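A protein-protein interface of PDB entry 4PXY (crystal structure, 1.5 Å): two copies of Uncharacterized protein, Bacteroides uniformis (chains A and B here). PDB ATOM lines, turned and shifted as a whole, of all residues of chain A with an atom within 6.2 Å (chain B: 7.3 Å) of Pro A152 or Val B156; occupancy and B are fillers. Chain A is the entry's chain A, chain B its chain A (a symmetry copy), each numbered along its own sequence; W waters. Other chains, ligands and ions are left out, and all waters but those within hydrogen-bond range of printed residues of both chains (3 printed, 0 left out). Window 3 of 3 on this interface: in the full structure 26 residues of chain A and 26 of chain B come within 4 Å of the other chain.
The side-chain amide oxygen (OD1) of Asn B185 is in hydrogen-bond range of the side-chain amide nitrogen (ND2) of Asn A150. The side-chain carboxylate of Asp B224 is in hydrogen-bond range of the backbone NH of Gly A225.
The backbone carbonyl oxygen (O) of Leu B137 is in hydrogen-bond range of the side-chain amide nitrogen (ND2) of Asn B185 (2.8 Å).
Among the printed residues, pairs that only touch across the chains: Asn A150 with Leu B137 (3.3 Å), Leu A229 with Pro B135 (3.4 Å), Leu A229 with Gln B134 (3.6 Å), Gly A225 with Val B156 (3.6 Å), Gly A225 with Pro B135 (3.6 Å), Thr A226 with Val B156 (3.7 Å), Pro A152 with Val B156 (3.9 Å) and Leu A229 with Val B156 (3.9 Å).
Printed residues of chain B within 4 Å of Asn A150: Leu B137 (3.3 Å) and Asn B185 (2.9 Å). Pro A152 touches just one residue of chain B: Val B156. Printed residues of chain B within 4 Å of Thr A226: Val B156. Printed residues of chain A within 4 Å of Leu B137: Asn A150 (3.3 Å). Of the printed residues of chain A, Asp B224 touches Gly A225. The nearest residue of chain B that does not touch Pro A152 is Leu B137 (4.8 Å). The nearest printed residue of chain B that does not touch Thr A226 is Asp B224 (4.8 Å).
Of the 15 printed residues of chain B, 6 touch a printed residue of chain A. Hydrophobic or aromatic side chains of chain B within 4 Å of the printed part of chain A: Pro B135, Leu B137 and Val B156. Printed residues of chain A that touch a printed residue of chain B: Asn A150, Pro A152, Gly A225, Thr A226 and Leu A229. Among the printed residues, 10 pairs touch across the chains.
5 positions are printed for both chains. Of the 10 pairs that touch across the chains among the printed residues, none has its exchanged pair printed and touching as well.
Water W1 lies within hydrogen-bond range of the side-chain carboxylate (OD2) of Asp B224 (2.7 Å), the backbone carbonyl oxygen (O) of Val B156 (2.9 Å), the backbone NH (N) of Thr A226 (3.1 Å) and the backbone NH (N) of Gly A225 (3.3 Å). Water W3 bridges N of Val B156 (2.9 Å) and OG1 of Thr A226 (3.1 Å). Water W2 bridges NE2 of Gln B134 and ND2 of Asn A150.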
ATOM      1  N   VAL A 138       5.489 -28.141  -3.982  1.00  0.00           N
ATOM      2  CA  VAL A 138       5.072 -27.287  -2.892  1.00  0.00           C
ATOM      3  C   VAL A 138       3.718 -27.765  -2.340  1.00  0.00           C
ATOM      4  O   VAL A 138       2.929 -28.386  -3.042  1.00  0.00           O
ATOM      5  CB  VAL A 138       5.004 -25.829  -3.348  1.00  0.00           C
ATOM      6  CG1 VAL A 138       6.322 -25.332  -3.904  1.00  0.00           C
ATOM      7  CG2 VAL A 138       3.928 -25.564  -4.302  1.00  0.00           C
ATOM      8  N   GLU A 139       3.491 -27.491  -1.063  1.00  0.00           N
ATOM      9  CA  GLU A 139       2.367 -27.960  -0.317  1.00  0.00           C
ATOM     10  C   GLU A 139       1.705 -26.764   0.351  1.00  0.00           C
ATOM     11  O   GLU A 139       2.379 -25.935   0.979  1.00  0.00           O
ATOM     12  CB  GLU A 139       2.830 -28.970   0.752  1.00  0.00           C
ATOM     13  CG  GLU A 139       3.227 -30.304   0.172  1.00  0.00           C
ATOM     14  CD  GLU A 139       4.094 -31.209   1.075  1.00  0.00           C
ATOM     15  OE1 GLU A 139       4.473 -30.816   2.207  1.00  0.00           O
ATOM     16  OE2 GLU A 139       4.446 -32.333   0.590  1.00  0.00           O
ATOM     17  N   VAL A 140       0.370 -26.723   0.300  1.00  0.00           N
ATOM     18  CA  VAL A 140      -0.408 -25.705   0.947  1.00  0.00           C
ATOM     19  C   VAL A 140      -0.554 -26.062   2.416  1.00  0.00           C
ATOM     20  O   VAL A 140      -1.052 -27.162   2.761  1.00  0.00           O
ATOM     21  CB  VAL A 140      -1.794 -25.607   0.274  1.00  0.00           C
ATOM     22  CG1 VAL A 140      -2.715 -24.739   1.087  1.00  0.00           C
ATOM     23  CG2 VAL A 140      -1.685 -25.033  -1.140  1.00  0.00           C
ATOM     24  N   THR A 148      -4.957 -19.397  -0.573  1.00  0.00           N
ATOM     25  CA  THR A 148      -4.715 -20.756  -1.083  1.00  0.00           C
ATOM     26  C   THR A 148      -5.991 -21.587  -1.282  1.00  0.00           C
ATOM     27  O   THR A 148      -5.878 -22.737  -1.715  1.00  0.00           O
ATOM     28  CB  THR A 148      -3.757 -21.480  -0.120  1.00  0.00           C
ATOM     29  OG1 THR A 148      -4.360 -21.469   1.157  1.00  0.00           O
ATOM     30  CG2 THR A 148      -2.375 -20.774  -0.112  1.00  0.00           C
ATOM     31  N   ASN A 150      -8.354 -21.708  -3.439  1.00  0.00           N
ATOM     32  CA  ASN A 150      -8.605 -22.171  -4.807  1.00  0.00           C
ATOM     33  C   ASN A 150      -7.323 -22.689  -5.465  1.00  0.00           C
ATOM     34  O   ASN A 150      -7.259 -22.779  -6.717  1.00  0.00           O
ATOM     35  CB  ASN A 150      -9.312 -21.094  -5.652  1.00  0.00           C
ATOM     36  CG  ASN A 150      -8.517 -19.832  -5.780  1.00  0.00           C
ATOM     37  OD1 ASN A 150      -7.534 -19.641  -5.063  1.00  0.00           O
ATOM     38  ND2 ASN A 150      -8.904 -18.982  -6.711  1.00  0.00           N
ATOM     39  N   LEU A 151      -6.310 -23.078  -4.681  1.00  0.00           N
ATOM     40  CA  LEU A 151      -5.132 -23.766  -5.186  1.00  0.00           C
ATOM     41  C   LEU A 151      -5.222 -25.262  -4.903  1.00  0.00           C
ATOM     42  O   LEU A 151      -5.772 -25.657  -3.881  1.00  0.00           O
ATOM     43  CB  LEU A 151      -3.849 -23.222  -4.561  1.00  0.00           C
ATOM     44  CG  LEU A 151      -3.622 -21.731  -4.765  1.00  0.00           C
ATOM     45  CD1 LEU A 151      -2.316 -21.351  -4.069  1.00  0.00           C
ATOM     46  CD2 LEU A 151      -3.566 -21.345  -6.243  1.00  0.00           C
ATOM     47  N   PRO A 152      -4.642 -26.094  -5.768  1.00  0.00           N
ATOM     48  CA  PRO A 152      -4.481 -27.501  -5.440  1.00  0.00           C
ATOM     49  C   PRO A 152      -3.654 -27.602  -4.128  1.00  0.00           C
ATOM     50  O   PRO A 152      -2.737 -26.802  -3.906  1.00  0.00           O
ATOM     51  CB  PRO A 152      -3.663 -28.067  -6.612  1.00  0.00           C
ATOM     52  CG  PRO A 152      -3.753 -27.021  -7.709  1.00  0.00           C
ATOM     53  CD  PRO A 152      -3.993 -25.708  -7.042  1.00  0.00           C
ATOM     54  N   ALA A 153      -3.922 -28.633  -3.329  1.00  0.00           N
ATOM     55  CA  ALA A 153      -3.222 -28.791  -2.031  1.00  0.00           C
ATOM     56  C   ALA A 153      -1.732 -28.990  -2.198  1.00  0.00           C
ATOM     57  O   ALA A 153      -0.967 -28.721  -1.312  1.00  0.00           O
ATOM     58  CB  ALA A 153      -3.812 -29.945  -1.260  1.00  0.00           C
ATOM     59  N   SER A 154      -1.318 -29.554  -3.315  1.00  0.00           N
ATOM     60  CA  SER A 154       0.118 -29.663  -3.654  1.00  0.00           C
ATOM     61  C   SER A 154       0.240 -29.497  -5.170  1.00  0.00           C
ATOM     62  O   SER A 154      -0.720 -29.788  -5.914  1.00  0.00           O
ATOM     63  CB  SER A 154       0.749 -30.954  -3.196  1.00  0.00           C
ATOM     64  OG  SER A 154       0.183 -32.004  -3.851  1.00  0.00           O
ATOM     65  N   PHE A 155       1.353 -28.931  -5.602  1.00  0.00           N
ATOM     66  CA  PHE A 155       1.624 -28.672  -7.013  1.00  0.00           C
ATOM     67  C   PHE A 155       3.072 -28.398  -7.186  1.00  0.00           C
ATOM     68  O   PHE A 155       3.785 -28.133  -6.241  1.00  0.00           O
ATOM     69  CB  PHE A 155       0.745 -27.506  -7.530  1.00  0.00           C
ATOM     70  CG  PHE A 155       0.965 -26.187  -6.874  1.00  0.00           C
ATOM     71  CD1 PHE A 155       0.233 -25.820  -5.761  1.00  0.00           C
ATOM     72  CD2 PHE A 155       1.861 -25.254  -7.429  1.00  0.00           C
ATOM     73  CE1 PHE A 155       0.415 -24.601  -5.159  1.00  0.00           C
ATOM     74  CE2 PHE A 155       2.026 -24.029  -6.850  1.00  0.00           C
ATOM     75  CZ  PHE A 155       1.285 -23.704  -5.686  1.00  0.00           C
ATOM     76  N   LEU A 179       2.449 -21.590   2.370  1.00  0.00           N
ATOM     77  CA  LEU A 179       2.954 -22.572   1.388  1.00  0.00           C
ATOM     78  C   LEU A 179       4.372 -22.962   1.807  1.00  0.00           C
ATOM     79  O   LEU A 179       5.146 -22.128   2.282  1.00  0.00           O
ATOM     80  CB  LEU A 179       2.939 -21.956  -0.012  1.00  0.00           C
ATOM     81  CG  LEU A 179       3.121 -22.829  -1.268  1.00  0.00           C
ATOM     82  CD1 LEU A 179       1.865 -23.563  -1.595  1.00  0.00           C
ATOM     83  CD2 LEU A 179       3.451 -22.016  -2.502  1.00  0.00           C
ATOM     84  N   GLY A 225      -0.210 -21.636 -14.755  1.00  0.00           N
ATOM     85  CA  GLY A 225      -1.424 -21.056 -14.189  1.00  0.00           C
ATOM     86  C   GLY A 225      -1.473 -21.125 -12.676  1.00  0.00           C
ATOM     87  O   GLY A 225      -1.898 -20.167 -12.028  1.00  0.00           O
ATOM     88  N   THR A 226      -1.083 -22.259 -12.095  1.00  0.00           N
ATOM     89  CA  THR A 226      -1.198 -22.426 -10.668  1.00  0.00           C
ATOM     90  C   THR A 226      -0.439 -21.396  -9.873  1.00  0.00           C
ATOM     91  O   THR A 226      -0.963 -20.750  -8.951  1.00  0.00           O
ATOM     92  CB  THR A 226      -0.815 -23.841 -10.185  1.00  0.00           C
ATOM     93  OG1 THR A 226      -1.489 -24.794 -11.028  1.00  0.00           O
ATOM     94  CG2 THR A 226      -1.208 -24.079  -8.727  1.00  0.00           C
ATOM     95  N   GLN A 227       0.862 -21.228 -10.185  1.00  0.00           N
ATOM     96  CA  GLN A 227       1.615 -20.219  -9.458  1.00  0.00           C
ATOM     97  C   GLN A 227       1.112 -18.809  -9.786  1.00  0.00           C
ATOM     98  O   GLN A 227       1.097 -17.935  -8.915  1.00  0.00           O
ATOM     99  CB  GLN A 227       3.116 -20.342  -9.742  1.00  0.00           C
ATOM    100  CG  GLN A 227       3.889 -19.404  -8.859  1.00  0.00           C
ATOM    101  CD  GLN A 227       5.371 -19.481  -9.131  1.00  0.00           C
ATOM    102  OE1 GLN A 227       6.079 -20.243  -8.490  1.00  0.00           O
ATOM    103  NE2 GLN A 227       5.855 -18.666 -10.075  1.00  0.00           N
ATOM    104  N   LEU A 229      -1.860 -17.969 -10.198  1.00  0.00           N
ATOM    105  CA  LEU A 229      -3.032 -17.790  -9.347  1.00  0.00           C
ATOM    106  C   LEU A 229      -2.651 -17.486  -7.908  1.00  0.00           C
ATOM    107  O   LEU A 229      -3.252 -16.606  -7.277  1.00  0.00           O
ATOM    108  CB  LEU A 229      -3.938 -19.030  -9.406  1.00  0.00           C
ATOM    109  CG  LEU A 229      -5.248 -18.934  -8.629  1.00  0.00           C
ATOM    110  CD1 LEU A 229      -5.985 -17.654  -8.928  1.00  0.00           C
ATOM    111  CD2 LEU A 229      -6.101 -20.167  -8.950  1.00  0.00           C
ATOM    112  N   GLN B 134      -7.740 -13.733 -15.225  1.00  0.00           N
ATOM    113  CA  GLN B 134      -6.884 -14.391 -14.239  1.00  0.00           C
ATOM    114  C   GLN B 134      -7.118 -15.894 -14.348  1.00  0.00           C
ATOM    115  O   GLN B 134      -8.178 -16.377 -14.781  1.00  0.00           O
ATOM    116  CB  GLN B 134      -7.183 -13.907 -12.821  1.00  0.00           C
ATOM    117  CG  GLN B 134      -8.584 -14.313 -12.318  1.00  0.00           C
ATOM    118  CD  GLN B 134      -8.673 -14.168 -10.816  1.00  0.00           C
ATOM    119  OE1 GLN B 134      -8.956 -13.103 -10.307  1.00  0.00           O
ATOM    120  NE2 GLN B 134      -8.320 -15.228 -10.102  1.00  0.00           N
ATOM    121  N   PRO B 135      -6.151 -16.663 -13.881  1.00  0.00           N
ATOM    122  CA  PRO B 135      -6.353 -18.113 -13.762  1.00  0.00           C
ATOM    123  C   PRO B 135      -7.401 -18.405 -12.689  1.00  0.00           C
ATOM    124  O   PRO B 135      -7.653 -17.583 -11.839  1.00  0.00           O
ATOM    125  CB  PRO B 135      -5.001 -18.667 -13.297  1.00  0.00           C
ATOM    126  CG  PRO B 135      -4.186 -17.497 -12.995  1.00  0.00           C
ATOM    127  CD  PRO B 135      -4.836 -16.239 -13.367  1.00  0.00           C
ATOM    128  N   VAL B 136      -8.002 -19.563 -12.775  1.00  0.00           N
ATOM    129  CA  VAL B 136      -9.024 -20.012 -11.847  1.00  0.00           C
ATOM    130  C   VAL B 136      -8.966 -21.498 -11.672  1.00  0.00           C
ATOM    131  O   VAL B 136      -8.537 -22.232 -12.585  1.00  0.00           O
ATOM    132  CB  VAL B 136     -10.437 -19.628 -12.276  1.00  0.00           C
ATOM    133  CG1 VAL B 136     -10.673 -18.106 -12.160  1.00  0.00           C
ATOM    134  CG2 VAL B 136     -10.736 -20.117 -13.688  1.00  0.00           C
ATOM    135  N   LEU B 137      -9.409 -21.980 -10.521  1.00  0.00           N
ATOM    136  CA  LEU B 137      -9.583 -23.398 -10.271  1.00  0.00           C
ATOM    137  C   LEU B 137     -10.838 -23.883 -11.028  1.00  0.00           C
ATOM    138  O   LEU B 137     -11.928 -23.324 -10.871  1.00  0.00           O
ATOM    139  CB  LEU B 137      -9.722 -23.715  -8.772  1.00  0.00           C
ATOM    140  CG  LEU B 137      -9.866 -25.171  -8.407  1.00  0.00           C
ATOM    141  CD1 LEU B 137      -8.557 -25.883  -8.661  1.00  0.00           C
ATOM    142  CD2 LEU B 137     -10.251 -25.288  -6.931  1.00  0.00           C
ATOM    143  N   VAL B 138     -10.696 -24.923 -11.819  1.00  0.00           N
ATOM    144  CA  VAL B 138     -11.795 -25.512 -12.552  1.00  0.00           C
ATOM    145  C   VAL B 138     -11.965 -26.986 -12.146  1.00  0.00           C
ATOM    146  O   VAL B 138     -11.023 -27.640 -11.715  1.00  0.00           O
ATOM    147  CB  VAL B 138     -11.573 -25.371 -14.058  1.00  0.00           C
ATOM    148  CG1 VAL B 138     -11.394 -23.929 -14.486  1.00  0.00           C
ATOM    149  CG2 VAL B 138     -10.467 -26.184 -14.564  1.00  0.00           C
ATOM    150  N   SER B 154      -9.677 -31.790 -11.048  1.00  0.00           N
ATOM    151  CA  SER B 154      -9.636 -30.326 -10.837  1.00  0.00           C
ATOM    152  C   SER B 154      -8.227 -29.855 -11.200  1.00  0.00           C
ATOM    153  O   SER B 154      -7.260 -30.642 -11.118  1.00  0.00           O
ATOM    154  CB  SER B 154     -10.006 -29.908  -9.436  1.00  0.00           C
ATOM    155  OG  SER B 154      -9.088 -30.387  -8.553  1.00  0.00           O
ATOM    156  N   PHE B 155      -8.135 -28.635 -11.700  1.00  0.00           N
ATOM    157  CA  PHE B 155      -6.873 -28.037 -12.124  1.00  0.00           C
ATOM    158  C   PHE B 155      -7.055 -26.572 -12.266  1.00  0.00           C
ATOM    159  O   PHE B 155      -8.159 -26.071 -12.320  1.00  0.00           O
ATOM    160  CB  PHE B 155      -6.374 -28.691 -13.436  1.00  0.00           C
ATOM    161  CG  PHE B 155      -7.262 -28.531 -14.620  1.00  0.00           C
ATOM    162  CD1 PHE B 155      -8.240 -29.465 -14.903  1.00  0.00           C
ATOM    163  CD2 PHE B 155      -7.064 -27.468 -15.522  1.00  0.00           C
ATOM    164  CE1 PHE B 155      -9.052 -29.337 -16.000  1.00  0.00           C
ATOM    165  CE2 PHE B 155      -7.853 -27.350 -16.630  1.00  0.00           C
ATOM    166  CZ  PHE B 155      -8.871 -28.308 -16.866  1.00  0.00           C
ATOM    167  N   VAL B 156      -5.947 -25.871 -12.313  1.00  0.00           N
ATOM    168  CA  VAL B 156      -5.995 -24.415 -12.514  1.00  0.00           C
ATOM    169  C   VAL B 156      -5.859 -24.174 -14.019  1.00  0.00           C
ATOM    170  O   VAL B 156      -4.862 -24.576 -14.603  1.00  0.00           O
ATOM    171  CB  VAL B 156      -4.912 -23.676 -11.726  1.00  0.00           C
ATOM    172  CG1 VAL B 156      -4.895 -22.207 -12.088  1.00  0.00           C
ATOM    173  CG2 VAL B 156      -5.156 -23.844 -10.234  1.00  0.00           C
ATOM    174  N   ALA B 157      -6.798 -23.437 -14.584  1.00  0.00           N
ATOM    175  CA  ALA B 157      -6.739 -23.044 -15.975  1.00  0.00           C
ATOM    176  C   ALA B 157      -6.035 -21.713 -16.054  1.00  0.00           C
ATOM    177  O   ALA B 157      -6.177 -20.864 -15.168  1.00  0.00           O
ATOM    178  CB  ALA B 157      -8.137 -22.862 -16.521  1.00  0.00           C
ATOM    179  N   PRO B 158      -5.288 -21.454 -17.129  1.00  0.00           N
ATOM    180  CA  PRO B 158      -4.646 -20.154 -17.300  1.00  0.00           C
ATOM    181  C   PRO B 158      -5.637 -19.022 -17.465  1.00  0.00           C
ATOM    182  O   PRO B 158      -6.859 -19.205 -17.582  1.00  0.00           O
ATOM    183  CB  PRO B 158      -3.793 -20.332 -18.558  1.00  0.00           C
ATOM    184  CG  PRO B 158      -4.034 -21.660 -19.058  1.00  0.00           C
ATOM    185  CD  PRO B 158      -4.952 -22.416 -18.184  1.00  0.00           C
ATOM    186  N   ALA B 159      -5.107 -17.812 -17.475  1.00  0.00           N
ATOM    187  CA  ALA B 159      -5.917 -16.632 -17.351  1.00  0.00           C
ATOM    188  C   ALA B 159      -6.899 -16.444 -18.503  1.00  0.00           C
ATOM    189  O   ALA B 159      -6.517 -16.543 -19.678  1.00  0.00           O
ATOM    190  CB  ALA B 159      -5.032 -15.389 -17.205  1.00  0.00           C
ATOM    191  N   ASN B 185     -13.259 -20.210  -6.001  1.00  0.00           N
ATOM    192  CA  ASN B 185     -12.691 -19.012  -6.573  1.00  0.00           C
ATOM    193  C   ASN B 185     -13.346 -17.682  -6.066  1.00  0.00           C
ATOM    194  O   ASN B 185     -12.781 -16.593  -6.257  1.00  0.00           O
ATOM    195  CB  ASN B 185     -12.756 -18.971  -8.088  1.00  0.00           C
ATOM    196  CG  ASN B 185     -11.921 -20.059  -8.762  1.00  0.00           C
ATOM    197  OD1 ASN B 185     -10.691 -20.026  -8.716  1.00  0.00           O
ATOM    198  ND2 ASN B 185     -12.595 -21.003  -9.369  1.00  0.00           N
ATOM    199  N   ASP B 224      -0.160 -24.040 -20.552  1.00  0.00           N
ATOM    200  CA  ASP B 224      -0.299 -25.258 -19.753  1.00  0.00           C
ATOM    201  C   ASP B 224      -0.817 -26.464 -20.541  1.00  0.00           C
ATOM    202  O   ASP B 224      -1.803 -26.410 -21.264  1.00  0.00           O
ATOM    203  CB  ASP B 224      -1.244 -25.044 -18.565  1.00  0.00           C
ATOM    204  CG  ASP B 224      -0.641 -24.127 -17.494  1.00  0.00           C
ATOM    205  OD1 ASP B 224       0.604 -23.934 -17.361  1.00  0.00           O
ATOM    206  OD2 ASP B 224      -1.451 -23.567 -16.722  1.00  0.00           O
ATOM    207  N   THR B 226      -2.420 -29.067 -19.431  1.00  0.00           N
ATOM    208  CA  THR B 226      -3.744 -29.511 -19.079  1.00  0.00           C
ATOM    209  C   THR B 226      -4.835 -28.879 -19.904  1.00  0.00           C
ATOM    210  O   THR B 226      -5.716 -29.549 -20.466  1.00  0.00           O
ATOM    211  CB  THR B 226      -4.067 -29.349 -17.579  1.00  0.00           C
ATOM    212  OG1 THR B 226      -2.960 -29.883 -16.828  1.00  0.00           O
ATOM    213  CG2 THR B 226      -5.352 -30.076 -17.182  1.00  0.00           C
ATOM    214  N   GLN B 227      -4.835 -27.532 -19.975  1.00  0.00           N
ATOM    215  CA  GLN B 227      -5.857 -26.891 -20.789  1.00  0.00           C
ATOM    216  C   GLN B 227      -5.659 -27.205 -22.276  1.00  0.00           C
ATOM    217  O   GLN B 227      -6.634 -27.353 -23.016  1.00  0.00           O
ATOM    218  CB  GLN B 227      -5.880 -25.378 -20.550  1.00  0.00           C
ATOM    219  CG  GLN B 227      -7.044 -24.757 -21.269  1.00  0.00           C
ATOM    220  CD  GLN B 227      -7.083 -23.261 -21.076  1.00  0.00           C
ATOM    221  OE1 GLN B 227      -7.729 -22.772 -20.163  1.00  0.00           O
ATOM    222  NE2 GLN B 227      -6.404 -22.521 -21.960  1.00  0.00           N
HETATM  223  O   HOH W   1      -1.975 -24.377 -14.199  1.00  0.00           O
HETATM  224  O   HOH W   2      -8.406 -16.065  -7.282  1.00  0.00           O
HETATM  225  O   HOH W   3      -3.459 -27.072 -11.589  1.00  0.00           O
